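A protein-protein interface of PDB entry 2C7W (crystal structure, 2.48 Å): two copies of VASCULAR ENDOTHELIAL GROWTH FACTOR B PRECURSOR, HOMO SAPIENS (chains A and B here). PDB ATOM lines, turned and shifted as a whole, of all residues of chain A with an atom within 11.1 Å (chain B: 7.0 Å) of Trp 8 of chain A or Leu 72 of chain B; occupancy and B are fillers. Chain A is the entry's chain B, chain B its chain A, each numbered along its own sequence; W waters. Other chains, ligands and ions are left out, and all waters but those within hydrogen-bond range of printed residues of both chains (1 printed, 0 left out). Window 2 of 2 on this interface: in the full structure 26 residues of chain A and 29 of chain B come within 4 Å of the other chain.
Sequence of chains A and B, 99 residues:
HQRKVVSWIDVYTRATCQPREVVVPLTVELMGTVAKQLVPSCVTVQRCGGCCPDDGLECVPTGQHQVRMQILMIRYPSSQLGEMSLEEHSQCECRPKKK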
ATOM      1  N   LYS A   4      12.188 -12.799 -13.229  1.00  0.00           N
ATOM      2  CA  LYS A   4      10.811 -13.166 -12.787  1.00  0.00           C
ATOM      3  C   LYS A   4       9.728 -12.448 -13.601  1.00  0.00           C
ATOM      4  O   LYS A   4       9.609 -11.217 -13.568  1.00  0.00           O
ATOM      5  CB  LYS A   4      10.620 -12.845 -11.301  1.00  0.00           C
ATOM      6  CG  LYS A   4       9.231 -13.227 -10.780  1.00  0.00           C
ATOM      7  CD  LYS A   4       9.011 -12.810  -9.322  1.00  0.00           C
ATOM      8  CE  LYS A   4       7.597 -13.183  -8.838  1.00  0.00           C
ATOM      9  NZ  LYS A   4       7.293 -12.720  -7.452  1.00  0.00           N
ATOM     10  N   VAL A   5       8.948 -13.236 -14.334  1.00  0.00           N
ATOM     11  CA  VAL A   5       7.867 -12.708 -15.154  1.00  0.00           C
ATOM     12  C   VAL A   5       6.544 -13.308 -14.702  1.00  0.00           C
ATOM     13  O   VAL A   5       6.409 -14.526 -14.601  1.00  0.00           O
ATOM     14  CB  VAL A   5       8.074 -13.042 -16.642  1.00  0.00           C
ATOM     15  CG1 VAL A   5       6.865 -12.604 -17.442  1.00  0.00           C
ATOM     16  CG2 VAL A   5       9.327 -12.351 -17.157  1.00  0.00           C
ATOM     17  N   VAL A   6       5.573 -12.447 -14.423  1.00  0.00           N
ATOM     18  CA  VAL A   6       4.264 -12.903 -13.986  1.00  0.00           C
ATOM     19  C   VAL A   6       3.263 -12.857 -15.147  1.00  0.00           C
ATOM     20  O   VAL A   6       3.116 -11.833 -15.823  1.00  0.00           O
ATOM     21  CB  VAL A   6       3.748 -12.048 -12.808  1.00  0.00           C
ATOM     22  CG1 VAL A   6       2.453 -12.635 -12.263  1.00  0.00           C
ATOM     23  CG2 VAL A   6       4.800 -11.998 -11.712  1.00  0.00           C
ATOM     24  N   SER A   7       2.594 -13.988 -15.369  1.00  0.00           N
ATOM     25  CA  SER A   7       1.604 -14.145 -16.432  1.00  0.00           C
ATOM     26  C   SER A   7       0.383 -13.239 -16.209  1.00  0.00           C
ATOM     27  O   SER A   7      -0.103 -13.099 -15.083  1.00  0.00           O
ATOM     28  CB  SER A   7       1.181 -15.616 -16.491  1.00  0.00           C
ATOM     29  OG  SER A   7       0.415 -15.899 -17.647  1.00  0.00           O
ATOM     30  N   TRP A   8      -0.108 -12.622 -17.281  1.00  0.00           N
ATOM     31  CA  TRP A   8      -1.265 -11.722 -17.197  1.00  0.00           C
ATOM     32  C   TRP A   8      -2.418 -12.276 -16.349  1.00  0.00           C
ATOM     33  O   TRP A   8      -2.996 -11.556 -15.535  1.00  0.00           O
ATOM     34  CB  TRP A   8      -1.787 -11.395 -18.596  1.00  0.00           C
ATOM     35  CG  TRP A   8      -2.988 -10.495 -18.586  1.00  0.00           C
ATOM     36  CD1 TRP A   8      -3.031  -9.175 -18.211  1.00  0.00           C
ATOM     37  CD2 TRP A   8      -4.327 -10.849 -18.955  1.00  0.00           C
ATOM     38  NE1 TRP A   8      -4.317  -8.687 -18.327  1.00  0.00           N
ATOM     39  CE2 TRP A   8      -5.131  -9.693 -18.779  1.00  0.00           C
ATOM     40  CE3 TRP A   8      -4.928 -12.030 -19.415  1.00  0.00           C
ATOM     41  CZ2 TRP A   8      -6.507  -9.687 -19.049  1.00  0.00           C
ATOM     42  CZ3 TRP A   8      -6.301 -12.025 -19.684  1.00  0.00           C
ATOM     43  CH2 TRP A   8      -7.071 -10.858 -19.498  1.00  0.00           C
ATOM     44  N   ILE A   9      -2.749 -13.548 -16.553  1.00  0.00           N
ATOM     45  CA  ILE A   9      -3.820 -14.196 -15.805  1.00  0.00           C
ATOM     46  C   ILE A   9      -3.586 -14.070 -14.316  1.00  0.00           C
ATOM     47  O   ILE A   9      -4.495 -13.711 -13.566  1.00  0.00           O
ATOM     48  CB  ILE A   9      -3.908 -15.688 -16.117  1.00  0.00           C
ATOM     49  CG1 ILE A   9      -2.498 -16.254 -16.275  1.00  0.00           C
ATOM     50  CG2 ILE A   9      -4.750 -15.917 -17.346  1.00  0.00           C
ATOM     51  CD1 ILE A   9      -2.451 -17.769 -16.453  1.00  0.00           C
ATOM     52  N   ASP A  10      -2.367 -14.383 -13.889  1.00  0.00           N
ATOM     53  CA  ASP A  10      -2.017 -14.299 -12.483  1.00  0.00           C
ATOM     54  C   ASP A  10      -2.049 -12.848 -12.032  1.00  0.00           C
ATOM     55  O   ASP A  10      -2.454 -12.547 -10.914  1.00  0.00           O
ATOM     56  CB  ASP A  10      -0.635 -14.899 -12.246  1.00  0.00           C
ATOM     57  CG  ASP A  10      -0.545 -16.349 -12.693  1.00  0.00           C
ATOM     58  OD1 ASP A  10      -0.698 -16.609 -13.910  1.00  0.00           O
ATOM     59  OD2 ASP A  10      -0.322 -17.233 -11.834  1.00  0.00           O
ATOM     60  N   VAL A  11      -1.642 -11.942 -12.906  1.00  0.00           N
ATOM     61  CA  VAL A  11      -1.642 -10.533 -12.558  1.00  0.00           C
ATOM     62  C   VAL A  11      -3.058 -10.001 -12.415  1.00  0.00           C
ATOM     63  O   VAL A  11      -3.362  -9.256 -11.482  1.00  0.00           O
ATOM     64  CB  VAL A  11      -0.932  -9.693 -13.616  1.00  0.00           C
ATOM     65  CG1 VAL A  11      -1.174  -8.215 -13.370  1.00  0.00           C
ATOM     66  CG2 VAL A  11       0.545  -9.988 -13.579  1.00  0.00           C
ATOM     67  N   TYR A  12      -3.913 -10.373 -13.360  1.00  0.00           N
ATOM     68  CA  TYR A  12      -5.290  -9.919 -13.356  1.00  0.00           C
ATOM     69  C   TYR A  12      -6.089 -10.491 -12.191  1.00  0.00           C
ATOM     70  O   TYR A  12      -6.630  -9.749 -11.380  1.00  0.00           O
ATOM     71  CB  TYR A  12      -5.974 -10.295 -14.671  1.00  0.00           C
ATOM     72  CG  TYR A  12      -7.315  -9.642 -14.805  1.00  0.00           C
ATOM     73  CD1 TYR A  12      -7.417  -8.257 -14.949  1.00  0.00           C
ATOM     74  CD2 TYR A  12      -8.491 -10.390 -14.724  1.00  0.00           C
ATOM     75  CE1 TYR A  12      -8.657  -7.630 -15.004  1.00  0.00           C
ATOM     76  CE2 TYR A  12      -9.739  -9.773 -14.780  1.00  0.00           C
ATOM     77  CZ  TYR A  12      -9.815  -8.393 -14.918  1.00  0.00           C
ATOM     78  OH  TYR A  12     -11.040  -7.772 -14.964  1.00  0.00           O
ATOM     79  N   THR A  13      -6.149 -11.815 -12.124  1.00  0.00           N
ATOM     80  CA  THR A  13      -6.883 -12.514 -11.082  1.00  0.00           C
ATOM     81  C   THR A  13      -6.514 -12.031  -9.696  1.00  0.00           C
ATOM     82  O   THR A  13      -7.337 -12.045  -8.775  1.00  0.00           O
ATOM     83  CB  THR A  13      -6.611 -14.017 -11.143  1.00  0.00           C
ATOM     84  OG1 THR A  13      -7.265 -14.568 -12.286  1.00  0.00           O
ATOM     85  CG2 THR A  13      -7.128 -14.713  -9.892  1.00  0.00           C
ATOM     86  N   ARG A  14      -5.274 -11.587  -9.559  1.00  0.00           N
ATOM     87  CA  ARG A  14      -4.762 -11.141  -8.280  1.00  0.00           C
ATOM     88  C   ARG A  14      -4.967  -9.667  -8.028  1.00  0.00           C
ATOM     89  O   ARG A  14      -5.022  -9.235  -6.886  1.00  0.00           O
ATOM     90  CB  ARG A  14      -3.278 -11.489  -8.200  1.00  0.00           C
ATOM     91  CG  ARG A  14      -2.693 -11.558  -6.812  1.00  0.00           C
ATOM     92  CD  ARG A  14      -1.328 -12.203  -6.912  1.00  0.00           C
ATOM     93  NE  ARG A  14      -1.395 -13.474  -7.635  1.00  0.00           N
ATOM     94  CZ  ARG A  14      -0.356 -14.063  -8.221  1.00  0.00           C
ATOM     95  NH1 ARG A  14       0.842 -13.496  -8.177  1.00  0.00           N
ATOM     96  NH2 ARG A  14      -0.512 -15.219  -8.858  1.00  0.00           N
ATOM     97  N   ALA A  15      -5.087  -8.886  -9.086  1.00  0.00           N
ATOM     98  CA  ALA A  15      -5.270  -7.456  -8.921  1.00  0.00           C
ATOM     99  C   ALA A  15      -6.761  -7.099  -8.922  1.00  0.00           C
ATOM    100  O   ALA A  15      -7.164  -5.992  -8.550  1.00  0.00           O
ATOM    101  CB  ALA A  15      -4.549  -6.721 -10.037  1.00  0.00           C
ATOM    102  N   THR A  16      -7.582  -8.048  -9.338  1.00  0.00           N
ATOM    103  CA  THR A  16      -9.002  -7.794  -9.396  1.00  0.00           C
ATOM    104  C   THR A  16      -9.664  -7.750  -8.019  1.00  0.00           C
ATOM    105  O   THR A  16      -9.386  -8.581  -7.139  1.00  0.00           O
ATOM    106  CB  THR A  16      -9.718  -8.831 -10.270  1.00  0.00           C
ATOM    107  OG1 THR A  16     -11.082  -8.433 -10.439  1.00  0.00           O
ATOM    108  CG2 THR A  16      -9.672 -10.196  -9.631  1.00  0.00           C
ATOM    109  N   GLN A  18     -11.243  -7.837  -4.644  1.00  0.00           N
ATOM    110  CA  GLN A  18     -11.516  -8.989  -3.798  1.00  0.00           C
ATOM    111  C   GLN A  18     -11.021  -8.673  -2.388  1.00  0.00           C
ATOM    112  O   GLN A  18     -10.392  -7.636  -2.153  1.00  0.00           O
ATOM    113  CB  GLN A  18     -10.788 -10.212  -4.338  1.00  0.00           C
ATOM    114  CG  GLN A  18      -9.266 -10.069  -4.279  1.00  0.00           C
ATOM    115  CD  GLN A  18      -8.563 -11.106  -5.115  1.00  0.00           C
ATOM    116  OE1 GLN A  18      -8.426 -12.261  -4.708  1.00  0.00           O
ATOM    117  NE2 GLN A  18      -8.129 -10.705  -6.307  1.00  0.00           N
ATOM    118  N   CYS A  51      -8.806  -3.472  -8.241  1.00  0.00           N
ATOM    119  CA  CYS A  51      -9.364  -2.532  -9.180  1.00  0.00           C
ATOM    120  C   CYS A  51     -10.522  -3.126  -9.959  1.00  0.00           C
ATOM    121  O   CYS A  51     -10.708  -4.345 -10.009  1.00  0.00           O
ATOM    122  CB  CYS A  51      -8.251  -2.004 -10.116  1.00  0.00           C
ATOM    123  SG  CYS A  51      -6.980  -3.226 -10.601  1.00  0.00           S
ATOM    124  N   PRO A  53     -12.799  -3.340 -13.625  1.00  0.00           N
ATOM    125  CA  PRO A  53     -12.738  -3.245 -15.086  1.00  0.00           C
ATOM    126  C   PRO A  53     -13.201  -1.891 -15.607  1.00  0.00           C
ATOM    127  O   PRO A  53     -13.146  -1.628 -16.806  1.00  0.00           O
ATOM    128  CB  PRO A  53     -13.651  -4.381 -15.534  1.00  0.00           C
ATOM    129  CG  PRO A  53     -13.398  -5.428 -14.480  1.00  0.00           C
ATOM    130  CD  PRO A  53     -13.435  -4.604 -13.206  1.00  0.00           C
ATOM    131  N   ALA B  35      -1.654   2.968 -25.142  1.00  0.00           N
ATOM    132  CA  ALA B  35      -2.850   2.320 -24.604  1.00  0.00           C
ATOM    133  C   ALA B  35      -3.492   3.132 -23.487  1.00  0.00           C
ATOM    134  O   ALA B  35      -3.046   3.096 -22.342  1.00  0.00           O
ATOM    135  CB  ALA B  35      -2.501   0.924 -24.096  1.00  0.00           C
ATOM    136  N   GLN B  37      -5.951   2.512 -22.079  1.00  0.00           N
ATOM    137  CA  GLN B  37      -6.617   1.569 -21.194  1.00  0.00           C
ATOM    138  C   GLN B  37      -5.715   0.403 -20.790  1.00  0.00           C
ATOM    139  O   GLN B  37      -5.334  -0.420 -21.620  1.00  0.00           O
ATOM    140  CB  GLN B  37      -7.885   1.038 -21.880  1.00  0.00           C
ATOM    141  CG  GLN B  37      -9.174   1.186 -21.063  1.00  0.00           C
ATOM    142  CD  GLN B  37      -9.276   0.180 -19.929  1.00  0.00           C
ATOM    143  OE1 GLN B  37      -9.353  -1.025 -20.160  1.00  0.00           O
ATOM    144  NE2 GLN B  37      -9.272   0.672 -18.698  1.00  0.00           N
ATOM    145  N   LEU B  38      -5.378   0.342 -19.506  1.00  0.00           N
ATOM    146  CA  LEU B  38      -4.544  -0.729 -18.977  1.00  0.00           C
ATOM    147  C   LEU B  38      -5.424  -1.738 -18.257  1.00  0.00           C
ATOM    148  O   LEU B  38      -6.329  -1.360 -17.519  1.00  0.00           O
ATOM    149  CB  LEU B  38      -3.501  -0.159 -18.016  1.00  0.00           C
ATOM    150  CG  LEU B  38      -2.088   0.029 -18.582  1.00  0.00           C
ATOM    151  CD1 LEU B  38      -2.124   0.545 -20.011  1.00  0.00           C
ATOM    152  CD2 LEU B  38      -1.335   0.985 -17.684  1.00  0.00           C
ATOM    153  N   VAL B  39      -5.156  -3.019 -18.481  1.00  0.00           N
ATOM    154  CA  VAL B  39      -5.930  -4.093 -17.872  1.00  0.00           C
ATOM    155  C   VAL B  39      -5.017  -5.209 -17.375  1.00  0.00           C
ATOM    156  O   VAL B  39      -4.429  -5.933 -18.175  1.00  0.00           O
ATOM    157  CB  VAL B  39      -6.930  -4.690 -18.895  1.00  0.00           C
ATOM    158  CG1 VAL B  39      -7.670  -5.884 -18.293  1.00  0.00           C
ATOM    159  CG2 VAL B  39      -7.905  -3.618 -19.340  1.00  0.00           C
ATOM    160  N   PRO B  40      -4.902  -5.379 -16.047  1.00  0.00           N
ATOM    161  CA  PRO B  40      -5.569  -4.593 -15.006  1.00  0.00           C
ATOM    162  C   PRO B  40      -5.024  -3.188 -14.836  1.00  0.00           C
ATOM    163  O   PRO B  40      -3.909  -2.878 -15.265  1.00  0.00           O
ATOM    164  CB  PRO B  40      -5.376  -5.443 -13.754  1.00  0.00           C
ATOM    165  CG  PRO B  40      -4.088  -6.140 -14.020  1.00  0.00           C
ATOM    166  CD  PRO B  40      -4.223  -6.546 -15.461  1.00  0.00           C
ATOM    167  N   MET B  69       5.574  -7.562 -14.726  1.00  0.00           N
ATOM    168  CA  MET B  69       4.128  -7.724 -14.669  1.00  0.00           C
ATOM    169  C   MET B  69       3.542  -7.684 -16.075  1.00  0.00           C
ATOM    170  O   MET B  69       3.620  -6.648 -16.716  1.00  0.00           O
ATOM    171  CB  MET B  69       3.529  -6.554 -13.879  1.00  0.00           C
ATOM    172  CG  MET B  69       2.688  -6.904 -12.677  1.00  0.00           C
ATOM    173  SD  MET B  69       3.628  -7.478 -11.274  1.00  0.00           S
ATOM    174  CE  MET B  69       3.619  -9.166 -11.583  1.00  0.00           C
ATOM    175  N   GLN B  70       2.976  -8.781 -16.573  1.00  0.00           N
ATOM    176  CA  GLN B  70       2.351  -8.715 -17.898  1.00  0.00           C
ATOM    177  C   GLN B  70       1.067  -7.897 -17.746  1.00  0.00           C
ATOM    178  O   GLN B  70       0.218  -8.212 -16.914  1.00  0.00           O
ATOM    179  CB  GLN B  70       2.030 -10.104 -18.445  1.00  0.00           C
ATOM    180  CG  GLN B  70       3.237 -10.805 -19.016  1.00  0.00           C
ATOM    181  CD  GLN B  70       2.914 -12.164 -19.590  1.00  0.00           C
ATOM    182  OE1 GLN B  70       1.631 -12.503 -19.620  1.00  0.00           O
ATOM    183  NE2 GLN B  70       3.806 -12.903 -20.005  1.00  0.00           N
ATOM    184  N   ILE B  71       0.951  -6.839 -18.543  1.00  0.00           N
ATOM    185  CA  ILE B  71      -0.193  -5.939 -18.490  1.00  0.00           C
ATOM    186  C   ILE B  71      -0.825  -5.727 -19.854  1.00  0.00           C
ATOM    187  O   ILE B  71      -0.168  -5.237 -20.762  1.00  0.00           O
ATOM    188  CB  ILE B  71       0.230  -4.561 -17.978  1.00  0.00           C
ATOM    189  CG1 ILE B  71       0.901  -4.705 -16.623  1.00  0.00           C
ATOM    190  CG2 ILE B  71      -0.974  -3.645 -17.887  1.00  0.00           C
ATOM    191  CD1 ILE B  71       0.076  -5.486 -15.636  1.00  0.00           C
ATOM    192  N   LEU B  72      -2.102  -6.072 -19.994  1.00  0.00           N
ATOM    193  CA  LEU B  72      -2.794  -5.886 -21.268  1.00  0.00           C
ATOM    194  C   LEU B  72      -2.967  -4.404 -21.572  1.00  0.00           C
ATOM    195  O   LEU B  72      -3.501  -3.654 -20.762  1.00  0.00           O
ATOM    196  CB  LEU B  72      -4.157  -6.575 -21.243  1.00  0.00           C
ATOM    197  CG  LEU B  72      -4.251  -7.651 -22.325  1.00  0.00           C
ATOM    198  CD1 LEU B  72      -5.490  -8.513 -22.136  1.00  0.00           C
ATOM    199  CD2 LEU B  72      -4.244  -6.967 -23.680  1.00  0.00           C
ATOM    200  N   MET B  73      -2.494  -3.982 -22.739  1.00  0.00           N
ATOM    201  CA  MET B  73      -2.601  -2.584 -23.132  1.00  0.00           C
ATOM    202  C   MET B  73      -3.666  -2.472 -24.202  1.00  0.00           C
ATOM    203  O   MET B  73      -3.808  -3.366 -25.047  1.00  0.00           O
ATOM    204  CB  MET B  73      -1.264  -2.073 -23.657  1.00  0.00           C
ATOM    205  CG  MET B  73      -0.136  -2.199 -22.651  1.00  0.00           C
ATOM    206  SD  MET B  73       1.379  -1.415 -23.205  1.00  0.00           S
ATOM    207  CE  MET B  73       1.916  -2.601 -24.440  1.00  0.00           C
ATOM    208  N   ILE B  74      -4.411  -1.372 -24.170  1.00  0.00           N
ATOM    209  CA  ILE B  74      -5.490  -1.184 -25.121  1.00  0.00           C
ATOM    210  C   ILE B  74      -5.664   0.197 -25.743  1.00  0.00           C
ATOM    211  O   ILE B  74      -5.576   1.229 -25.076  1.00  0.00           O
ATOM    212  CB  ILE B  74      -6.835  -1.608 -24.480  1.00  0.00           C
ATOM    213  CG1 ILE B  74      -6.836  -3.123 -24.251  1.00  0.00           C
ATOM    214  CG2 ILE B  74      -8.002  -1.195 -25.363  1.00  0.00           C
ATOM    215  CD1 ILE B  74      -8.141  -3.665 -23.725  1.00  0.00           C
ATOM    216  N   SER B  78      -7.356  -2.628 -31.161  1.00  0.00           N
ATOM    217  CA  SER B  78      -7.141  -3.887 -30.456  1.00  0.00           C
ATOM    218  C   SER B  78      -6.170  -3.728 -29.279  1.00  0.00           C
ATOM    219  O   SER B  78      -5.774  -2.612 -28.933  1.00  0.00           O
ATOM    220  CB  SER B  78      -6.656  -4.972 -31.415  1.00  0.00           C
ATOM    221  OG  SER B  78      -7.363  -6.186 -31.182  1.00  0.00           O
ATOM    222  N   SER B  79      -5.805  -4.843 -28.654  1.00  0.00           N
ATOM    223  CA  SER B  79      -4.908  -4.778 -27.515  1.00  0.00           C
ATOM    224  C   SER B  79      -3.796  -5.806 -27.539  1.00  0.00           C
ATOM    225  O   SER B  79      -3.912  -6.858 -28.173  1.00  0.00           O
ATOM    226  N   GLN B  80      -2.714  -5.507 -26.836  1.00  0.00           N
ATOM    227  CA  GLN B  80      -1.580  -6.413 -26.795  1.00  0.00           C
ATOM    228  C   GLN B  80      -0.946  -6.443 -25.412  1.00  0.00           C
ATOM    229  O   GLN B  80      -0.954  -5.447 -24.685  1.00  0.00           O
ATOM    230  CB  GLN B  80      -0.529  -5.986 -27.824  1.00  0.00           C
ATOM    231  CG  GLN B  80       0.235  -4.731 -27.417  1.00  0.00           C
ATOM    232  CD  GLN B  80       1.337  -4.366 -28.394  1.00  0.00           C
ATOM    233  OE1 GLN B  80       2.163  -5.206 -28.767  1.00  0.00           O
ATOM    234  NE2 GLN B  80       1.359  -3.101 -28.809  1.00  0.00           N
ATOM    235  N   LEU B  81      -0.392  -7.595 -25.064  1.00  0.00           N
ATOM    236  CA  LEU B  81       0.267  -7.778 -23.781  1.00  0.00           C
ATOM    237  C   LEU B  81       1.537  -6.960 -23.655  1.00  0.00           C
ATOM    238  O   LEU B  81       2.461  -7.085 -24.456  1.00  0.00           O
ATOM    239  CB  LEU B  81       0.602  -9.253 -23.561  1.00  0.00           C
ATOM    240  CG  LEU B  81      -0.593 -10.144 -23.231  1.00  0.00           C
ATOM    241  CD1 LEU B  81      -0.161 -11.607 -23.210  1.00  0.00           C
ATOM    242  CD2 LEU B  81      -1.177  -9.710 -21.877  1.00  0.00           C
ATOM    243  N   GLY B  82       1.558  -6.107 -22.643  1.00  0.00           N
ATOM    244  CA  GLY B  82       2.715  -5.284 -22.370  1.00  0.00           C
ATOM    245  C   GLY B  82       3.401  -5.912 -21.176  1.00  0.00           C
ATOM    246  O   GLY B  82       3.032  -7.001 -20.745  1.00  0.00           O
ATOM    247  N   GLU B  83       4.396  -5.239 -20.628  1.00  0.00           N
ATOM    248  CA  GLU B  83       5.098  -5.798 -19.492  1.00  0.00           C
ATOM    249  C   GLU B  83       5.669  -4.656 -18.693  1.00  0.00           C
ATOM    250  O   GLU B  83       6.634  -4.005 -19.111  1.00  0.00           O
ATOM    251  CB  GLU B  83       6.220  -6.712 -19.971  1.00  0.00           C
ATOM    252  CG  GLU B  83       6.371  -7.976 -19.163  1.00  0.00           C
ATOM    253  CD  GLU B  83       7.370  -8.933 -19.788  1.00  0.00           C
ATOM    254  OE1 GLU B  83       8.578  -8.594 -19.832  1.00  0.00           O
ATOM    255  OE2 GLU B  83       6.943 -10.021 -20.239  1.00  0.00           O
HETATM  256  O   HOH W   1       1.709 -15.007 -20.357  1.00  0.00           O
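The backbone NH (N) of Val 39 of chain B sits at hydrogen-bond distance from the backbone carbonyl oxygen (O) of Leu 72 of chain B. O of Ile 71 of chain B lies within hydrogen-bond range of N of Gly 82 of chain B (2.7 Å).
Of the 16 printed residues of chain A, 6 touch a printed residue of chain B. Printed residues of chain A that touch a printed residue of chain B: Val 5, Val 6, Ser 7, Trp 8, Val 11 and Tyr 12. Hydrophobic or aromatic side chains of chain A within 4 Å of the printed part of chain B: Val 5, Val 6, Trp 8, Val 11 and Tyr 12. Along chain A the printed residues that touch a printed residue of chain B span positions 5 to 12. Of the 17 printed residues of chain B, 8 touch a printed residue of chain A. Among the printed residues, no Asp or Glu carboxylate lies within 4 Å of a Lys or Arg side-chain nitrogen of the other chain.
Water W1 bridges the side-chain amide oxygen (OE1) of Gln 70 of chain B (2.6 Å) and the side-chain hydroxyl (OG) of Ser 7 of chain A (3.1 Å).
Printed residues of chain B within 4 Å of Val 6 of chain A: Met 69 (3.1 Å) and Gln 70 (3.1 Å). Printed residues of chain B within 4 Å of Ser 7 of chain A: Gln 70. Trp 8 of chain A touches just these residues of chain B: Val 39 (2.8 Å), Pro 40 (3.6 Å), Gln 70 (2.9 Å), Leu 72 (3.5 Å) and Leu 81 (3.7 Å). Pro 53 of chain A touches none of the printed residues of chain B. No residue of chain A comes within 4 Å of Leu 38 of chain B. Val 39 of chain B touches just these residues of chain A: Trp 8 and Tyr 12. Printed residues of chain A within 4 Å of Pro 40 of chain B: Trp 8, Val 11 and Tyr 12. Of the printed residues of chain A, Met 69 of chain B touches Val 6 (3.1 Å) and Val 11 (3.8 Å). Printed residues of chain A within 4 Å of Gln 70 of chain B: Val 6, Ser 7, Trp 8 and Val 11. Of chain A, only Val 11 comes within 4 Å of Ile 71 of chain B. Leu 72 of chain B touches just one residue of chain A: Trp 8. No residue of chain A comes within 4 Å of Ile 74 of chain B. Of chain A, only Trp 8 (3.7 Å) comes within 4 Å of Leu 81 of chain B. The nearest residue of chain A that does not touch Leu 72 of chain B is Val 11 of chain A (7.0 Å). The nearest printed residue of chain A that does not touch Gln 70 of chain B is Val 5 of chain A (4.002 Å).
O of Val 39 of chain B sits at hydrogen-bond distance from NE1 of Trp 8 of chain A (2.8 Å). The backbone NH (N) of Gln 70 of chain B lies within hydrogen-bond range of the backbone carbonyl oxygen (O) of Val 6 of chain A (3.1 Å). The side-chain amide oxygen of Gln 70 of chain B is in hydrogen-bond range of the backbone NH of Trp 8 of chain A.
No position is printed for both chains.
Among the printed residues, pairs that only touch across the chains: Val 5 of chain A with Glu 83 of chain B, Val 6 of chain A with Met 69 of chain B, Ser 7 of chain A with Gln 70 of chain B, Trp 8 of chain A with Pro 40 of chain B, Trp 8 of chain A with Leu 72 of chain B, Trp 8 of chain A with Leu 81 of chain B, Val 11 of chain A with Pro 40 of chain B, Val 11 of chain A with Met 69 of chain B, Val 11 of chain A with Gln 70 of chain B, Val 11 of chain A with Ile 71 of chain B, Tyr 12 of chain A with Val 39 of chain B and Tyr 12 of chain A with Pro 40 of chain B.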
